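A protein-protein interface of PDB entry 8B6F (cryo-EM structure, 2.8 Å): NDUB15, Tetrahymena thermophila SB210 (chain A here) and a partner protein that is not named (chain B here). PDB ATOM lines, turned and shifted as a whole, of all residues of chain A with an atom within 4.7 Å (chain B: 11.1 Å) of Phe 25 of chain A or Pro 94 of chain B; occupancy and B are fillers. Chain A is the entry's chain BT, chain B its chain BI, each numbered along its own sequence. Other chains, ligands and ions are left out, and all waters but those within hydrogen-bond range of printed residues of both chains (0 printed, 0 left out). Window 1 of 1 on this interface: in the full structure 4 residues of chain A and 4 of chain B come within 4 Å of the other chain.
Lys 93 of chain B touches Glu 23 of chain A (CB to CG, 3.7 Å). O of Phe 24 of chain A touches CG of Pro 94 of chain B, 3.8 Å away. Phe 25 of chain A touches Pro 94 of chain B. Phe 25 of chain A touches Asp 96 of chain B (CE1 to CA, 3.9 Å). Asn 59 of chain A touches Pro 97 of chain B (OD1 to CD, 3.4 Å).
Of the 8 printed residues of chain A, 4 touch a printed residue of chain B. Hydrophobic or aromatic side chains of chain A that line the printed part of chain B: Phe 25. Printed residues of chain B that touch a printed residue of chain A: Lys 93, Pro 94, Asp 96 and Pro 97. Hydrophobic or aromatic side chains of chain B that line the printed part of chain A: Pro 94 and Pro 97. Among the printed residues, no Asp or Glu carboxylate lies within 4 Å of a Lys or Arg side-chain nitrogen of the other chain.
The side-chain amino group (NZ) of Lys 93 of chain B lies within salt-bridge range of the side-chain carboxylate (OE2) of Glu 150 of chain B (2.7 Å). The side-chain carboxylate of Asp 96 of chain B lies within hydrogen-bond range of the side-chain amide nitrogen of Asn 88 of chain B (3.4 Å). N of Val 98 of chain B sits at hydrogen-bond distance from OD1 of Asp 96 of chain B, 2.9 Å away.
Asn 26 of chain A touches none of the printed residues of chain B. No residue of chain B comes within 4 Å of Val 51 of chain A. No residue of chain B comes within 4 Å of Phe 55 of chain A. Of the printed residues of chain B, Asn 59 of chain A touches Pro 97. Of the printed residues of chain A, Lys 93 of chain B touches Glu 23. Pro 94 of chain B touches just these residues of chain A: Phe 24 (3.8 Å) and Phe 25 (3.7 Å). Of the printed residues of chain A, Asp 96 of chain B touches Phe 25 (3.9 Å). Of the printed residues of chain A, Pro 97 of chain B touches Asn 59. Cys 146 of chain B touches none of the printed residues of chain A. The nearest residue of chain B that does not touch Phe 25 of chain A is Ile 95 of chain B (4.1 Å). The nearest residue of chain A that does not touch Pro 94 of chain B is Glu 23 of chain A (4.1 Å).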
ATOM      1  N   GLU A  23     -22.798  -3.575  28.984  1.00  0.00           N
ATOM      2  CA  GLU A  23     -22.203  -4.901  29.057  1.00  0.00           C
ATOM      3  C   GLU A  23     -21.166  -4.940  30.168  1.00  0.00           C
ATOM      4  O   GLU A  23     -20.366  -4.011  30.318  1.00  0.00           O
ATOM      5  CB  GLU A  23     -21.555  -5.294  27.726  1.00  0.00           C
ATOM      6  CG  GLU A  23     -22.528  -5.339  26.556  1.00  0.00           C
ATOM      7  CD  GLU A  23     -22.706  -3.992  25.883  1.00  0.00           C
ATOM      8  OE1 GLU A  23     -21.977  -3.042  26.239  1.00  0.00           O
ATOM      9  OE2 GLU A  23     -23.577  -3.882  24.994  1.00  0.00           O
ATOM     10  N   PHE A  24     -21.182  -6.022  30.940  1.00  0.00           N
ATOM     11  CA  PHE A  24     -20.242  -6.206  32.036  1.00  0.00           C
ATOM     12  C   PHE A  24     -20.174  -7.689  32.366  1.00  0.00           C
ATOM     13  O   PHE A  24     -21.109  -8.446  32.092  1.00  0.00           O
ATOM     14  CB  PHE A  24     -20.660  -5.399  33.270  1.00  0.00           C
ATOM     15  CG  PHE A  24     -22.080  -5.639  33.695  1.00  0.00           C
ATOM     16  CD1 PHE A  24     -23.119  -4.933  33.115  1.00  0.00           C
ATOM     17  CD2 PHE A  24     -22.375  -6.568  34.676  1.00  0.00           C
ATOM     18  CE1 PHE A  24     -24.426  -5.151  33.502  1.00  0.00           C
ATOM     19  CE2 PHE A  24     -23.681  -6.793  35.068  1.00  0.00           C
ATOM     20  CZ  PHE A  24     -24.707  -6.083  34.480  1.00  0.00           C
ATOM     21  N   PHE A  25     -19.053  -8.098  32.953  1.00  0.00           N
ATOM     22  CA  PHE A  25     -18.911  -9.482  33.383  1.00  0.00           C
ATOM     23  C   PHE A  25     -19.954  -9.812  34.442  1.00  0.00           C
ATOM     24  O   PHE A  25     -20.271  -8.987  35.303  1.00  0.00           O
ATOM     25  CB  PHE A  25     -17.505  -9.730  33.929  1.00  0.00           C
ATOM     26  CG  PHE A  25     -16.418  -9.511  32.919  1.00  0.00           C
ATOM     27  CD1 PHE A  25     -16.133 -10.477  31.970  1.00  0.00           C
ATOM     28  CD2 PHE A  25     -15.674  -8.345  32.925  1.00  0.00           C
ATOM     29  CE1 PHE A  25     -15.132 -10.281  31.041  1.00  0.00           C
ATOM     30  CE2 PHE A  25     -14.669  -8.143  31.999  1.00  0.00           C
ATOM     31  CZ  PHE A  25     -14.399  -9.112  31.056  1.00  0.00           C
ATOM     32  N   ASN A  26     -20.491 -11.026  34.371  1.00  0.00           N
ATOM     33  CA  ASN A  26     -21.589 -11.452  35.224  1.00  0.00           C
ATOM     34  C   ASN A  26     -21.297 -12.829  35.801  1.00  0.00           C
ATOM     35  O   ASN A  26     -20.413 -13.550  35.330  1.00  0.00           O
ATOM     36  CB  ASN A  26     -22.914 -11.490  34.451  1.00  0.00           C
ATOM     37  CG  ASN A  26     -23.984 -10.630  35.087  1.00  0.00           C
ATOM     38  OD1 ASN A  26     -24.451  -9.663  34.490  1.00  0.00           O
ATOM     39  ND2 ASN A  26     -24.385 -10.984  36.301  1.00  0.00           N
ATOM     40  N   TYR A  27     -22.045 -13.180  36.844  1.00  0.00           N
ATOM     41  CA  TYR A  27     -21.967 -14.523  37.397  1.00  0.00           C
ATOM     42  C   TYR A  27     -22.359 -15.551  36.343  1.00  0.00           C
ATOM     43  O   TYR A  27     -23.346 -15.384  35.624  1.00  0.00           O
ATOM     44  CB  TYR A  27     -22.887 -14.657  38.610  1.00  0.00           C
ATOM     45  CG  TYR A  27     -22.458 -13.854  39.813  1.00  0.00           C
ATOM     46  CD1 TYR A  27     -22.767 -12.506  39.920  1.00  0.00           C
ATOM     47  CD2 TYR A  27     -21.760 -14.451  40.853  1.00  0.00           C
ATOM     48  CE1 TYR A  27     -22.383 -11.772  41.024  1.00  0.00           C
ATOM     49  CE2 TYR A  27     -21.372 -13.727  41.960  1.00  0.00           C
ATOM     50  CZ  TYR A  27     -21.687 -12.388  42.039  1.00  0.00           C
ATOM     51  OH  TYR A  27     -21.301 -11.664  43.144  1.00  0.00           O
ATOM     52  N   VAL A  51     -22.183  -5.495  40.143  1.00  0.00           N
ATOM     53  CA  VAL A  51     -21.630  -6.671  39.474  1.00  0.00           C
ATOM     54  C   VAL A  51     -20.355  -6.304  38.728  1.00  0.00           C
ATOM     55  O   VAL A  51     -19.377  -7.061  38.728  1.00  0.00           O
ATOM     56  CB  VAL A  51     -22.673  -7.305  38.537  1.00  0.00           C
ATOM     57  CG1 VAL A  51     -22.105  -8.551  37.880  1.00  0.00           C
ATOM     58  CG2 VAL A  51     -23.930  -7.659  39.303  1.00  0.00           C
ATOM     59  N   PHE A  55     -16.544  -8.055  39.393  1.00  0.00           N
ATOM     60  CA  PHE A  55     -15.751  -8.792  38.419  1.00  0.00           C
ATOM     61  C   PHE A  55     -14.686  -7.946  37.734  1.00  0.00           C
ATOM     62  O   PHE A  55     -13.985  -8.461  36.859  1.00  0.00           O
ATOM     63  CB  PHE A  55     -16.677  -9.417  37.374  1.00  0.00           C
ATOM     64  CG  PHE A  55     -17.426 -10.611  37.881  1.00  0.00           C
ATOM     65  CD1 PHE A  55     -16.842 -11.866  37.868  1.00  0.00           C
ATOM     66  CD2 PHE A  55     -18.707 -10.477  38.388  1.00  0.00           C
ATOM     67  CE1 PHE A  55     -17.524 -12.964  38.344  1.00  0.00           C
ATOM     68  CE2 PHE A  55     -19.394 -11.571  38.866  1.00  0.00           C
ATOM     69  CZ  PHE A  55     -18.803 -12.817  38.842  1.00  0.00           C
ATOM     70  N   ASN A  59     -10.425  -9.312  36.170  1.00  0.00           N
ATOM     71  CA  ASN A  59     -10.116  -9.193  34.753  1.00  0.00           C
ATOM     72  C   ASN A  59      -9.174  -8.040  34.427  1.00  0.00           C
ATOM     73  O   ASN A  59      -8.735  -7.932  33.277  1.00  0.00           O
ATOM     74  CB  ASN A  59     -11.413  -9.027  33.955  1.00  0.00           C
ATOM     75  CG  ASN A  59     -12.389 -10.157  34.199  1.00  0.00           C
ATOM     76  OD1 ASN A  59     -12.311 -11.210  33.567  1.00  0.00           O
ATOM     77  ND2 ASN A  59     -13.319  -9.945  35.121  1.00  0.00           N
ATOM     78  N   ILE B  87     -17.521 -22.871  27.106  1.00  0.00           N
ATOM     79  CA  ILE B  87     -17.422 -21.916  28.202  1.00  0.00           C
ATOM     80  C   ILE B  87     -16.405 -20.852  27.823  1.00  0.00           C
ATOM     81  O   ILE B  87     -15.440 -21.120  27.099  1.00  0.00           O
ATOM     82  CB  ILE B  87     -17.036 -22.593  29.537  1.00  0.00           C
ATOM     83  CG1 ILE B  87     -15.740 -23.391  29.379  1.00  0.00           C
ATOM     84  CG2 ILE B  87     -18.171 -23.488  30.013  1.00  0.00           C
ATOM     85  CD1 ILE B  87     -15.218 -23.989  30.672  1.00  0.00           C
ATOM     86  N   ASN B  88     -16.619 -19.636  28.323  1.00  0.00           N
ATOM     87  CA  ASN B  88     -15.789 -18.491  27.953  1.00  0.00           C
ATOM     88  C   ASN B  88     -15.767 -18.310  26.438  1.00  0.00           C
ATOM     89  O   ASN B  88     -14.724 -18.053  25.836  1.00  0.00           O
ATOM     90  CB  ASN B  88     -14.370 -18.641  28.501  1.00  0.00           C
ATOM     91  CG  ASN B  88     -14.348 -18.888  29.993  1.00  0.00           C
ATOM     92  OD1 ASN B  88     -13.848 -19.912  30.456  1.00  0.00           O
ATOM     93  ND2 ASN B  88     -14.892 -17.949  30.757  1.00  0.00           N
ATOM     94  N   THR B  89     -16.935 -18.448  25.820  1.00  0.00           N
ATOM     95  CA  THR B  89     -17.033 -18.409  24.372  1.00  0.00           C
ATOM     96  C   THR B  89     -16.797 -16.994  23.850  1.00  0.00           C
ATOM     97  O   THR B  89     -16.874 -16.007  24.585  1.00  0.00           O
ATOM     98  CB  THR B  89     -18.407 -18.896  23.911  1.00  0.00           C
ATOM     99  OG1 THR B  89     -19.409 -17.950  24.299  1.00  0.00           O
ATOM    100  CG2 THR B  89     -18.737 -20.232  24.543  1.00  0.00           C
ATOM    101  N   MET B  90     -16.498 -16.911  22.553  1.00  0.00           N
ATOM    102  CA  MET B  90     -16.307 -15.625  21.897  1.00  0.00           C
ATOM    103  C   MET B  90     -17.608 -14.852  21.726  1.00  0.00           C
ATOM    104  O   MET B  90     -17.563 -13.669  21.377  1.00  0.00           O
ATOM    105  CB  MET B  90     -15.662 -15.835  20.528  1.00  0.00           C
ATOM    106  CG  MET B  90     -14.266 -16.426  20.589  1.00  0.00           C
ATOM    107  SD  MET B  90     -13.046 -15.282  21.256  1.00  0.00           S
ATOM    108  CE  MET B  90     -13.015 -14.038  19.972  1.00  0.00           C
ATOM    109  N   LEU B  91     -18.757 -15.490  21.953  1.00  0.00           N
ATOM    110  CA  LEU B  91     -20.042 -14.827  21.784  1.00  0.00           C
ATOM    111  C   LEU B  91     -20.403 -13.918  22.947  1.00  0.00           C
ATOM    112  O   LEU B  91     -21.263 -13.044  22.786  1.00  0.00           O
ATOM    113  CB  LEU B  91     -21.140 -15.874  21.595  1.00  0.00           C
ATOM    114  CG  LEU B  91     -20.989 -16.771  20.368  1.00  0.00           C
ATOM    115  CD1 LEU B  91     -22.061 -17.841  20.354  1.00  0.00           C
ATOM    116  CD2 LEU B  91     -21.051 -15.945  19.098  1.00  0.00           C
ATOM    117  N   GLU B  92     -19.783 -14.098  24.108  1.00  0.00           N
ATOM    118  CA  GLU B  92     -20.040 -13.208  25.229  1.00  0.00           C
ATOM    119  C   GLU B  92     -19.618 -11.792  24.867  1.00  0.00           C
ATOM    120  O   GLU B  92     -18.515 -11.575  24.358  1.00  0.00           O
ATOM    121  CB  GLU B  92     -19.286 -13.693  26.465  1.00  0.00           C
ATOM    122  CG  GLU B  92     -19.649 -15.111  26.878  1.00  0.00           C
ATOM    123  CD  GLU B  92     -18.733 -15.659  27.951  1.00  0.00           C
ATOM    124  OE1 GLU B  92     -17.766 -14.963  28.323  1.00  0.00           O
ATOM    125  OE2 GLU B  92     -18.980 -16.790  28.420  1.00  0.00           O
ATOM    126  N   LYS B  93     -20.499 -10.826  25.127  1.00  0.00           N
ATOM    127  CA  LYS B  93     -20.213  -9.453  24.713  1.00  0.00           C
ATOM    128  C   LYS B  93     -18.926  -8.933  25.332  1.00  0.00           C
ATOM    129  O   LYS B  93     -18.042  -8.484  24.582  1.00  0.00           O
ATOM    130  CB  LYS B  93     -21.406  -8.552  25.047  1.00  0.00           C
ATOM    131  CG  LYS B  93     -22.571  -8.684  24.077  1.00  0.00           C
ATOM    132  CD  LYS B  93     -22.202  -8.170  22.693  1.00  0.00           C
ATOM    133  CE  LYS B  93     -23.426  -8.060  21.804  1.00  0.00           C
ATOM    134  NZ  LYS B  93     -23.074  -7.602  20.429  1.00  0.00           N
ATOM    135  N   PRO B  94     -18.746  -8.952  26.651  1.00  0.00           N
ATOM    136  CA  PRO B  94     -17.404  -8.778  27.222  1.00  0.00           C
ATOM    137  C   PRO B  94     -16.658 -10.100  27.180  1.00  0.00           C
ATOM    138  O   PRO B  94     -16.978 -11.035  27.920  1.00  0.00           O
ATOM    139  CB  PRO B  94     -17.697  -8.321  28.657  1.00  0.00           C
ATOM    140  CG  PRO B  94     -18.991  -8.969  28.984  1.00  0.00           C
ATOM    141  CD  PRO B  94     -19.780  -9.031  27.700  1.00  0.00           C
ATOM    142  N   ILE B  95     -15.665 -10.188  26.301  1.00  0.00           N
ATOM    143  CA  ILE B  95     -14.969 -11.450  26.077  1.00  0.00           C
ATOM    144  C   ILE B  95     -14.002 -11.675  27.232  1.00  0.00           C
ATOM    145  O   ILE B  95     -13.150 -10.830  27.521  1.00  0.00           O
ATOM    146  CB  ILE B  95     -14.237 -11.448  24.728  1.00  0.00           C
ATOM    147  CG1 ILE B  95     -15.221 -11.098  23.605  1.00  0.00           C
ATOM    148  CG2 ILE B  95     -13.590 -12.807  24.481  1.00  0.00           C
ATOM    149  CD1 ILE B  95     -14.630 -11.121  22.209  1.00  0.00           C
ATOM    150  N   ASP B  96     -14.136 -12.817  27.892  1.00  0.00           N
ATOM    151  CA  ASP B  96     -13.296 -13.122  29.041  1.00  0.00           C
ATOM    152  C   ASP B  96     -11.845 -13.271  28.593  1.00  0.00           C
ATOM    153  O   ASP B  96     -11.577 -13.962  27.606  1.00  0.00           O
ATOM    154  CB  ASP B  96     -13.778 -14.400  29.720  1.00  0.00           C
ATOM    155  CG  ASP B  96     -13.146 -14.609  31.081  1.00  0.00           C
ATOM    156  OD1 ASP B  96     -11.917 -14.436  31.205  1.00  0.00           O
ATOM    157  OD2 ASP B  96     -13.881 -14.948  32.031  1.00  0.00           O
ATOM    158  N   PRO B  97     -10.885 -12.651  29.285  1.00  0.00           N
ATOM    159  CA  PRO B  97      -9.482 -12.777  28.853  1.00  0.00           C
ATOM    160  C   PRO B  97      -8.938 -14.195  28.913  1.00  0.00           C
ATOM    161  O   PRO B  97      -7.907 -14.467  28.288  1.00  0.00           O
ATOM    162  CB  PRO B  97      -8.731 -11.847  29.818  1.00  0.00           C
ATOM    163  CG  PRO B  97      -9.632 -11.688  30.985  1.00  0.00           C
ATOM    164  CD  PRO B  97     -11.019 -11.745  30.437  1.00  0.00           C
ATOM    165  N   VAL B  98      -9.585 -15.104  29.641  1.00  0.00           N
ATOM    166  CA  VAL B  98      -9.085 -16.468  29.780  1.00  0.00           C
ATOM    167  C   VAL B  98      -9.659 -17.341  28.670  1.00  0.00           C
ATOM    168  O   VAL B  98      -9.512 -18.567  28.691  1.00  0.00           O
ATOM    169  CB  VAL B  98      -9.419 -17.043  31.171  1.00  0.00           C
ATOM    170  CG1 VAL B  98     -10.889 -17.447  31.271  1.00  0.00           C
ATOM    171  CG2 VAL B  98      -8.511 -18.220  31.496  1.00  0.00           C
ATOM    172  N   THR B  99     -10.318 -16.722  27.695  1.00  0.00           N
ATOM    173  CA  THR B  99     -10.867 -17.474  26.577  1.00  0.00           C
ATOM    174  C   THR B  99      -9.749 -17.992  25.683  1.00  0.00           C
ATOM    175  O   THR B  99      -8.728 -17.328  25.491  1.00  0.00           O
ATOM    176  CB  THR B  99     -11.823 -16.598  25.766  1.00  0.00           C
ATOM    177  OG1 THR B  99     -12.486 -17.394  24.777  1.00  0.00           O
ATOM    178  CG2 THR B  99     -11.072 -15.471  25.065  1.00  0.00           C
ATOM    179  N   HIS B 123     -10.791  -9.348  17.493  1.00  0.00           N
ATOM    180  CA  HIS B 123     -10.097  -9.906  18.641  1.00  0.00           C
ATOM    181  C   HIS B 123      -8.762 -10.486  18.191  1.00  0.00           C
ATOM    182  O   HIS B 123      -8.605 -10.918  17.047  1.00  0.00           O
ATOM    183  CB  HIS B 123     -10.957 -10.986  19.298  1.00  0.00           C
ATOM    184  CG  HIS B 123     -10.557 -11.314  20.702  1.00  0.00           C
ATOM    185  ND1 HIS B 123      -9.731 -12.372  21.013  1.00  0.00           N
ATOM    186  CD2 HIS B 123     -10.881 -10.732  21.881  1.00  0.00           C
ATOM    187  CE1 HIS B 123      -9.560 -12.424  22.321  1.00  0.00           C
ATOM    188  NE2 HIS B 123     -10.248 -11.441  22.871  1.00  0.00           N
ATOM    189  N   CYS B 146     -17.474 -16.546  15.792  1.00  0.00           N
ATOM    190  CA  CYS B 146     -17.158 -15.345  16.557  1.00  0.00           C
ATOM    191  C   CYS B 146     -18.188 -14.231  16.373  1.00  0.00           C
ATOM    192  O   CYS B 146     -18.243 -13.319  17.204  1.00  0.00           O
ATOM    193  CB  CYS B 146     -15.772 -14.822  16.181  1.00  0.00           C
ATOM    194  SG  CYS B 146     -14.436 -15.995  16.491  1.00  0.00           S
ATOM    195  N   LEU B 148     -21.849 -12.668  16.573  1.00  0.00           N
ATOM    196  CA  LEU B 148     -23.113 -12.812  17.286  1.00  0.00           C
ATOM    197  C   LEU B 148     -24.168 -11.963  16.590  1.00  0.00           C
ATOM    198  O   LEU B 148     -23.930 -10.787  16.298  1.00  0.00           O
ATOM    199  CB  LEU B 148     -22.971 -12.385  18.747  1.00  0.00           C
ATOM    200  CG  LEU B 148     -24.245 -12.445  19.593  1.00  0.00           C
ATOM    201  CD1 LEU B 148     -24.786 -13.858  19.654  1.00  0.00           C
ATOM    202  CD2 LEU B 148     -23.975 -11.921  20.986  1.00  0.00           C
ATOM    203  N   GLU B 150     -27.146  -9.601  15.716  1.00  0.00           N
ATOM    204  CA  GLU B 150     -27.726  -8.419  16.333  1.00  0.00           C
ATOM    205  C   GLU B 150     -28.809  -7.854  15.424  1.00  0.00           C
ATOM    206  O   GLU B 150     -28.857  -8.147  14.227  1.00  0.00           O
ATOM    207  CB  GLU B 150     -26.662  -7.347  16.599  1.00  0.00           C
ATOM    208  CG  GLU B 150     -25.644  -7.731  17.657  1.00  0.00           C
ATOM    209  CD  GLU B 150     -26.245  -7.794  19.046  1.00  0.00           C
ATOM    210  OE1 GLU B 150     -27.382  -7.309  19.226  1.00  0.00           O
ATOM    211  OE2 GLU B 150     -25.583  -8.328  19.957  1.00  0.00           O
